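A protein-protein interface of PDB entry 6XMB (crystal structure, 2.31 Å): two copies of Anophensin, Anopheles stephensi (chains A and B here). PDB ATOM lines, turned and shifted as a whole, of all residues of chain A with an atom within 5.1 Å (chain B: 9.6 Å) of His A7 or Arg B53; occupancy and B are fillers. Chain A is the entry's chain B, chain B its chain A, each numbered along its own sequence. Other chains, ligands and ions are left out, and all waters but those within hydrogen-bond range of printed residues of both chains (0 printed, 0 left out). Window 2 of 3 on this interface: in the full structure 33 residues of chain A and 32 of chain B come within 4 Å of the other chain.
The side-chain hydroxyl of Thr A4 sits at hydrogen-bond distance from the backbone carbonyl oxygen of Met B49 (3.4 Å). The backbone carbonyl oxygen (O) of Pro B52 lies within hydrogen-bond range of a ring nitrogen (NE2) of His A7 (3.1 Å).
The side-chain amino group of Lys A6 is in hydrogen-bond range of the side-chain amide oxygen of Gln A10 (3.1 Å).
Thr A4 touches Ala B48 (OG1 to O, 3.7 Å). Thr A4 touches Leu B51. His A7 touches Ala B48. His A7 touches Leu B51. Ala B55 touches His A7. Val A8 touches Met B49 (CG2 to CG, 3.5 Å). Leu B44 touches Leu A11 (O to CD1, 3.4 Å). CE1 of Tyr B45 touches CB of Leu A11, at 3.8 Å. CB of Ala B48 touches CD1 of Leu A11, 3.6 Å away. Leu A11 touches Leu B62 (CD2 to CD2, 3.6 Å).
No residue of chain B comes within 4 Å of Lys A6. Of the printed residues of chain B, His A7 touches Ala B48, Leu B51, Pro B52, Arg B53 and Ala B55. Val A8 touches one residue of chain B. Of the printed residues of chain A, Tyr B45 touches Leu A11. Of the printed residues of chain A, Ala B48 touches Thr A4 (3.7 Å), His A7 (3.9 Å) and Leu A11 (3.6 Å). Of the printed residues of chain A, Met B49 touches Thr A4 and Val A8. Ser B50 touches none of the printed residues of chain A. Printed residues of chain A within 4 Å of Pro B52: His A7. The nearest printed residue of chain A that does not touch Arg B53 is Thr A4 (4.1 Å). The nearest printed residue of chain A that does not touch Leu B57 is His A7 (4.3 Å).
Of the 19 printed residues of chain B, 10 touch a printed residue of chain A. Hydrophobic or aromatic side chains of chain B that line the printed part of chain A: Tyr B45, Ala B48, Met B49, Leu B51, Leu B57 and Leu B62. Of the 9 printed residues of chain A, 5 touch a printed residue of chain B. Hydrophobic or aromatic side chains of chain A that line the printed part of chain B: His A7, Val A8 and Leu A11.
No position is printed for both chains.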
ATOM      1  N   ALA A   3       6.482  27.438  -0.007  1.00  0.00           N
ATOM      2  CA  ALA A   3       7.779  28.108  -0.004  1.00  0.00           C
ATOM      3  C   ALA A   3       8.743  27.436  -0.982  1.00  0.00           C
ATOM      4  O   ALA A   3       9.440  28.105  -1.744  1.00  0.00           O
ATOM      5  CB  ALA A   3       8.368  28.125   1.405  1.00  0.00           C
ATOM      6  N   THR A   4       8.793  26.104  -0.945  1.00  0.00           N
ATOM      7  CA  THR A   4       9.569  25.309  -1.900  1.00  0.00           C
ATOM      8  C   THR A   4       8.690  24.177  -2.434  1.00  0.00           C
ATOM      9  O   THR A   4       8.982  22.989  -2.285  1.00  0.00           O
ATOM     10  CB  THR A   4      10.851  24.739  -1.295  1.00  0.00           C
ATOM     11  OG1 THR A   4      10.525  23.673  -0.390  1.00  0.00           O
ATOM     12  CG2 THR A   4      11.637  25.837  -0.567  1.00  0.00           C
ATOM     13  N   ARG A   5       7.578  24.571  -3.057  1.00  0.00           N
ATOM     14  CA  ARG A   5       6.711  23.620  -3.738  1.00  0.00           C
ATOM     15  C   ARG A   5       7.433  22.913  -4.883  1.00  0.00           C
ATOM     16  O   ARG A   5       7.026  21.817  -5.283  1.00  0.00           O
ATOM     17  CB  ARG A   5       5.465  24.359  -4.245  1.00  0.00           C
ATOM     18  CG  ARG A   5       4.328  23.482  -4.737  1.00  0.00           C
ATOM     19  CD  ARG A   5       3.610  22.759  -3.598  1.00  0.00           C
ATOM     20  NE  ARG A   5       3.706  21.305  -3.724  1.00  0.00           N
ATOM     21  CZ  ARG A   5       2.944  20.439  -3.059  1.00  0.00           C
ATOM     22  NH1 ARG A   5       2.015  20.882  -2.220  1.00  0.00           N
ATOM     23  NH2 ARG A   5       3.103  19.132  -3.239  1.00  0.00           N
ATOM     24  N   LYS A   6       8.526  23.497  -5.386  1.00  0.00           N
ATOM     25  CA  LYS A   6       9.150  23.008  -6.613  1.00  0.00           C
ATOM     26  C   LYS A   6       9.849  21.673  -6.389  1.00  0.00           C
ATOM     27  O   LYS A   6       9.618  20.711  -7.126  1.00  0.00           O
ATOM     28  CB  LYS A   6      10.135  24.054  -7.152  1.00  0.00           C
ATOM     29  CG  LYS A   6      10.503  23.865  -8.620  1.00  0.00           C
ATOM     30  CD  LYS A   6      11.693  22.926  -8.788  1.00  0.00           C
ATOM     31  CE  LYS A   6      11.701  22.245 -10.158  1.00  0.00           C
ATOM     32  NZ  LYS A   6      10.706  21.132 -10.277  1.00  0.00           N
ATOM     33  N   HIS A   7      10.729  21.598  -5.389  1.00  0.00           N
ATOM     34  CA  HIS A   7      11.459  20.356  -5.155  1.00  0.00           C
ATOM     35  C   HIS A   7      10.525  19.215  -4.771  1.00  0.00           C
ATOM     36  O   HIS A   7      10.800  18.059  -5.102  1.00  0.00           O
ATOM     37  CB  HIS A   7      12.507  20.550  -4.064  1.00  0.00           C
ATOM     38  CG  HIS A   7      13.253  21.845  -4.162  1.00  0.00           C
ATOM     39  ND1 HIS A   7      13.459  22.499  -5.359  1.00  0.00           N
ATOM     40  CD2 HIS A   7      13.829  22.616  -3.208  1.00  0.00           C
ATOM     41  CE1 HIS A   7      14.133  23.615  -5.136  1.00  0.00           C
ATOM     42  NE2 HIS A   7      14.371  23.709  -3.839  1.00  0.00           N
ATOM     43  N   VAL A   8       9.424  19.512  -4.080  1.00  0.00           N
ATOM     44  CA  VAL A   8       8.516  18.455  -3.647  1.00  0.00           C
ATOM     45  C   VAL A   8       7.777  17.863  -4.838  1.00  0.00           C
ATOM     46  O   VAL A   8       7.714  16.640  -5.001  1.00  0.00           O
ATOM     47  CB  VAL A   8       7.531  18.985  -2.596  1.00  0.00           C
ATOM     48  CG1 VAL A   8       6.755  17.817  -1.998  1.00  0.00           C
ATOM     49  CG2 VAL A   8       8.270  19.777  -1.527  1.00  0.00           C
ATOM     50  N   GLN A   9       7.188  18.721  -5.676  1.00  0.00           N
ATOM     51  CA  GLN A   9       6.527  18.227  -6.878  1.00  0.00           C
ATOM     52  C   GLN A   9       7.490  17.411  -7.726  1.00  0.00           C
ATOM     53  O   GLN A   9       7.105  16.391  -8.306  1.00  0.00           O
ATOM     54  CB  GLN A   9       5.962  19.380  -7.702  1.00  0.00           C
ATOM     55  CG  GLN A   9       4.837  20.150  -7.061  1.00  0.00           C
ATOM     56  CD  GLN A   9       4.179  21.090  -8.061  1.00  0.00           C
ATOM     57  OE1 GLN A   9       4.342  20.934  -9.275  1.00  0.00           O
ATOM     58  NE2 GLN A   9       3.438  22.071  -7.559  1.00  0.00           N
ATOM     59  N   GLN A  10       8.752  17.841  -7.801  1.00  0.00           N
ATOM     60  CA  GLN A  10       9.735  17.108  -8.591  1.00  0.00           C
ATOM     61  C   GLN A  10      10.015  15.731  -8.002  1.00  0.00           C
ATOM     62  O   GLN A  10      10.211  14.767  -8.751  1.00  0.00           O
ATOM     63  CB  GLN A  10      11.027  17.918  -8.704  1.00  0.00           C
ATOM     64  CG  GLN A  10      12.103  17.317  -9.603  1.00  0.00           C
ATOM     65  CD  GLN A  10      13.327  18.237  -9.740  1.00  0.00           C
ATOM     66  OE1 GLN A  10      13.207  19.468  -9.689  1.00  0.00           O
ATOM     67  NE2 GLN A  10      14.504  17.641  -9.902  1.00  0.00           N
ATOM     68  N   LEU A  11      10.030  15.613  -6.672  1.00  0.00           N
ATOM     69  CA  LEU A  11      10.210  14.300  -6.058  1.00  0.00           C
ATOM     70  C   LEU A  11       8.964  13.438  -6.196  1.00  0.00           C
ATOM     71  O   LEU A  11       9.071  12.211  -6.297  1.00  0.00           O
ATOM     72  CB  LEU A  11      10.577  14.437  -4.581  1.00  0.00           C
ATOM     73  CG  LEU A  11      12.058  14.558  -4.245  1.00  0.00           C
ATOM     74  CD1 LEU A  11      12.272  14.464  -2.748  1.00  0.00           C
ATOM     75  CD2 LEU A  11      12.826  13.469  -4.964  1.00  0.00           C
ATOM     76  N   LEU B  44      12.762  11.275   2.319  1.00  0.00           N
ATOM     77  CA  LEU B  44      13.249  12.175   1.274  1.00  0.00           C
ATOM     78  C   LEU B  44      12.290  13.330   1.039  1.00  0.00           C
ATOM     79  O   LEU B  44      12.709  14.399   0.591  1.00  0.00           O
ATOM     80  CB  LEU B  44      13.469  11.416  -0.030  1.00  0.00           C
ATOM     81  CG  LEU B  44      14.771  10.631  -0.154  1.00  0.00           C
ATOM     82  CD1 LEU B  44      14.648   9.643  -1.297  1.00  0.00           C
ATOM     83  CD2 LEU B  44      15.939  11.577  -0.414  1.00  0.00           C
ATOM     84  N   TYR B  45      11.001  13.136   1.315  1.00  0.00           N
ATOM     85  CA  TYR B  45      10.094  14.276   1.282  1.00  0.00           C
ATOM     86  C   TYR B  45      10.459  15.293   2.348  1.00  0.00           C
ATOM     87  O   TYR B  45      10.253  16.494   2.147  1.00  0.00           O
ATOM     88  CB  TYR B  45       8.645  13.833   1.473  1.00  0.00           C
ATOM     89  CG  TYR B  45       7.953  13.377   0.204  1.00  0.00           C
ATOM     90  CD1 TYR B  45       8.480  13.676  -1.049  1.00  0.00           C
ATOM     91  CD2 TYR B  45       6.759  12.656   0.256  1.00  0.00           C
ATOM     92  CE1 TYR B  45       7.839  13.258  -2.224  1.00  0.00           C
ATOM     93  CE2 TYR B  45       6.115  12.245  -0.905  1.00  0.00           C
ATOM     94  CZ  TYR B  45       6.658  12.547  -2.134  1.00  0.00           C
ATOM     95  OH  TYR B  45       6.021  12.135  -3.275  1.00  0.00           O
ATOM     96  N   LEU B  46      10.991  14.832   3.487  1.00  0.00           N
ATOM     97  CA  LEU B  46      11.430  15.747   4.535  1.00  0.00           C
ATOM     98  C   LEU B  46      12.576  16.611   4.045  1.00  0.00           C
ATOM     99  O   LEU B  46      12.548  17.840   4.183  1.00  0.00           O
ATOM    100  CB  LEU B  46      11.850  14.967   5.781  1.00  0.00           C
ATOM    101  CG  LEU B  46      10.766  14.134   6.485  1.00  0.00           C
ATOM    102  CD1 LEU B  46      11.361  13.321   7.630  1.00  0.00           C
ATOM    103  CD2 LEU B  46       9.656  15.013   7.006  1.00  0.00           C
ATOM    104  N   LYS B  47      13.593  15.978   3.464  1.00  0.00           N
ATOM    105  CA  LYS B  47      14.743  16.704   2.953  1.00  0.00           C
ATOM    106  C   LYS B  47      14.330  17.741   1.922  1.00  0.00           C
ATOM    107  O   LYS B  47      14.877  18.847   1.892  1.00  0.00           O
ATOM    108  CB  LYS B  47      15.732  15.714   2.358  1.00  0.00           C
ATOM    109  CG  LYS B  47      17.049  16.331   1.898  1.00  0.00           C
ATOM    110  CD  LYS B  47      17.939  16.649   3.089  1.00  0.00           C
ATOM    111  CE  LYS B  47      19.402  16.807   2.673  1.00  0.00           C
ATOM    112  NZ  LYS B  47      20.264  17.002   3.883  1.00  0.00           N
ATOM    113  N   ALA B  48      13.365  17.407   1.069  1.00  0.00           N
ATOM    114  CA  ALA B  48      13.011  18.298  -0.027  1.00  0.00           C
ATOM    115  C   ALA B  48      12.385  19.585   0.486  1.00  0.00           C
ATOM    116  O   ALA B  48      12.658  20.670  -0.038  1.00  0.00           O
ATOM    117  CB  ALA B  48      12.053  17.592  -0.983  1.00  0.00           C
ATOM    118  N   MET B  49      11.533  19.481   1.505  1.00  0.00           N
ATOM    119  CA  MET B  49      10.797  20.647   1.975  1.00  0.00           C
ATOM    120  C   MET B  49      11.682  21.592   2.763  1.00  0.00           C
ATOM    121  O   MET B  49      11.455  22.805   2.745  1.00  0.00           O
ATOM    122  CB  MET B  49       9.600  20.202   2.808  1.00  0.00           C
ATOM    123  CG  MET B  49       8.356  20.029   1.980  1.00  0.00           C
ATOM    124  SD  MET B  49       7.018  19.326   2.943  1.00  0.00           S
ATOM    125  CE  MET B  49       6.781  20.594   4.195  1.00  0.00           C
ATOM    126  N   SER B  50      12.683  21.059   3.459  1.00  0.00           N
ATOM    127  CA  SER B  50      13.710  21.876   4.092  1.00  0.00           C
ATOM    128  C   SER B  50      14.880  22.000   3.119  1.00  0.00           C
ATOM    129  O   SER B  50      15.892  21.311   3.225  1.00  0.00           O
ATOM    130  CB  SER B  50      14.140  21.260   5.415  1.00  0.00           C
ATOM    131  OG  SER B  50      15.042  20.177   5.211  1.00  0.00           O
ATOM    132  N   LEU B  51      14.712  22.877   2.136  1.00  0.00           N
ATOM    133  CA  LEU B  51      15.748  23.176   1.158  1.00  0.00           C
ATOM    134  C   LEU B  51      15.594  24.622   0.715  1.00  0.00           C
ATOM    135  O   LEU B  51      14.469  25.129   0.646  1.00  0.00           O
ATOM    136  CB  LEU B  51      15.660  22.255  -0.068  1.00  0.00           C
ATOM    137  CG  LEU B  51      16.462  20.952  -0.160  1.00  0.00           C
ATOM    138  CD1 LEU B  51      16.221  20.314  -1.522  1.00  0.00           C
ATOM    139  CD2 LEU B  51      17.940  21.174   0.051  1.00  0.00           C
ATOM    140  N   PRO B  52      16.694  25.297   0.390  1.00  0.00           N
ATOM    141  CA  PRO B  52      16.593  26.680  -0.088  1.00  0.00           C
ATOM    142  C   PRO B  52      15.845  26.771  -1.410  1.00  0.00           C
ATOM    143  O   PRO B  52      15.949  25.895  -2.271  1.00  0.00           O
ATOM    144  CB  PRO B  52      18.058  27.109  -0.249  1.00  0.00           C
ATOM    145  CG  PRO B  52      18.826  25.830  -0.389  1.00  0.00           C
ATOM    146  CD  PRO B  52      18.090  24.835   0.466  1.00  0.00           C
ATOM    147  N   ARG B  53      15.067  27.851  -1.551  1.00  0.00           N
ATOM    148  CA  ARG B  53      14.371  28.111  -2.807  1.00  0.00           C
ATOM    149  C   ARG B  53      15.318  27.988  -3.992  1.00  0.00           C
ATOM    150  O   ARG B  53      14.915  27.537  -5.070  1.00  0.00           O
ATOM    151  CB  ARG B  53      13.724  29.502  -2.777  1.00  0.00           C
ATOM    152  N   SER B  54      16.578  28.367  -3.811  1.00  0.00           N
ATOM    153  CA  SER B  54      17.561  28.299  -4.888  1.00  0.00           C
ATOM    154  C   SER B  54      18.486  27.102  -4.667  1.00  0.00           C
ATOM    155  O   SER B  54      19.665  27.217  -4.332  1.00  0.00           O
ATOM    156  CB  SER B  54      18.332  29.614  -4.988  1.00  0.00           C
ATOM    157  OG  SER B  54      19.111  29.850  -3.833  1.00  0.00           O
ATOM    158  N   ALA B  55      17.910  25.923  -4.864  1.00  0.00           N
ATOM    159  CA  ALA B  55      18.654  24.673  -4.884  1.00  0.00           C
ATOM    160  C   ALA B  55      18.274  23.903  -6.139  1.00  0.00           C
ATOM    161  O   ALA B  55      17.104  23.879  -6.529  1.00  0.00           O
ATOM    162  CB  ALA B  55      18.375  23.824  -3.639  1.00  0.00           C
ATOM    163  N   LYS B  56      19.270  23.313  -6.792  1.00  0.00           N
ATOM    164  CA  LYS B  56      19.057  22.495  -7.977  1.00  0.00           C
ATOM    165  C   LYS B  56      19.238  21.030  -7.605  1.00  0.00           C
ATOM    166  O   LYS B  56      20.157  20.678  -6.860  1.00  0.00           O
ATOM    167  CB  LYS B  56      20.023  22.886  -9.099  1.00  0.00           C
ATOM    168  N   LEU B  57      18.350  20.184  -8.110  1.00  0.00           N
ATOM    169  CA  LEU B  57      18.356  18.769  -7.770  1.00  0.00           C
ATOM    170  C   LEU B  57      19.217  17.986  -8.745  1.00  0.00           C
ATOM    171  O   LEU B  57      19.173  18.213  -9.957  1.00  0.00           O
ATOM    172  CB  LEU B  57      16.936  18.203  -7.775  1.00  0.00           C
ATOM    173  CG  LEU B  57      16.042  18.542  -6.584  1.00  0.00           C
ATOM    174  CD1 LEU B  57      14.815  17.647  -6.615  1.00  0.00           C
ATOM    175  CD2 LEU B  57      16.794  18.386  -5.277  1.00  0.00           C
ATOM    176  N   SER B  58      19.994  17.051  -8.208  1.00  0.00           N
ATOM    177  CA  SER B  58      20.869  16.213  -9.020  1.00  0.00           C
ATOM    178  C   SER B  58      20.050  15.083  -9.634  1.00  0.00           C
ATOM    179  O   SER B  58      19.672  14.134  -8.939  1.00  0.00           O
ATOM    180  CB  SER B  58      22.009  15.657  -8.172  1.00  0.00           C
ATOM    181  OG  SER B  58      22.769  14.697  -8.892  1.00  0.00           O
ATOM    182  N   LEU B  62      18.712  11.057  -8.604  1.00  0.00           N
ATOM    183  CA  LEU B  62      17.401  10.424  -8.709  1.00  0.00           C
ATOM    184  C   LEU B  62      17.471   9.185  -9.585  1.00  0.00           C
ATOM    185  O   LEU B  62      16.798   8.182  -9.313  1.00  0.00           O
ATOM    186  CB  LEU B  62      16.378  11.413  -9.269  1.00  0.00           C
ATOM    187  CG  LEU B  62      16.121  12.674  -8.444  1.00  0.00           C
ATOM    188  CD1 LEU B  62      15.227  13.631  -9.213  1.00  0.00           C
ATOM    189  CD2 LEU B  62      15.505  12.329  -7.089  1.00  0.00           C
ATOM    190  N   LEU B 117      21.457  14.670  -3.211  1.00  0.00           N
ATOM    191  CA  LEU B 117      20.218  15.218  -3.759  1.00  0.00           C
ATOM    192  C   LEU B 117      20.427  16.607  -4.360  1.00  0.00           C
ATOM    193  O   LEU B 117      19.971  16.887  -5.475  1.00  0.00           O
ATOM    194  CB  LEU B 117      19.150  15.259  -2.673  1.00  0.00           C
ATOM    195  CG  LEU B 117      17.742  15.513  -3.200  1.00  0.00           C
ATOM    196  CD1 LEU B 117      17.326  14.413  -4.163  1.00  0.00           C
ATOM    197  CD2 LEU B 117      16.790  15.602  -2.037  1.00  0.00           C
ATOM    198  N   VAL B 118      21.101  17.494  -3.634  1.00  0.00           N
ATOM    199  CA  VAL B 118      21.325  18.863  -4.096  1.00  0.00           C
ATOM    200  C   VAL B 118      22.496  18.887  -5.072  1.00  0.00           C
ATOM    201  O   VAL B 118      23.572  18.354  -4.772  1.00  0.00           O
ATOM    202  CB  VAL B 118      21.596  19.797  -2.904  1.00  0.00           C
ATOM    203  CG1 VAL B 118      21.430  21.260  -3.309  1.00  0.00           C
ATOM    204  CG2 VAL B 118      20.714  19.442  -1.723  1.00  0.00           C
ATOM    205  N   GLN B 119      22.269  19.471  -6.255  1.00  0.00           N
ATOM    206  CA  GLN B 119      23.318  20.074  -7.111  1.00  0.00           C
ATOM    207  C   GLN B 119      22.740  20.514  -8.460  1.00  0.00           C
ATOM    208  O   GLN B 119      22.733  19.751  -9.430  1.00  0.00           O
ATOM    209  CB  GLN B 119      24.499  19.130  -7.350  1.00  0.00           C
ATOM    210  CG  GLN B 119      25.828  19.840  -7.554  1.00  0.00           C
ATOM    211  CD  GLN B 119      26.194  20.764  -6.399  1.00  0.00           C
ATOM    212  OE1 GLN B 119      25.723  20.593  -5.273  1.00  0.00           O
ATOM    213  NE2 GLN B 119      27.040  21.755  -6.680  1.00  0.00           N
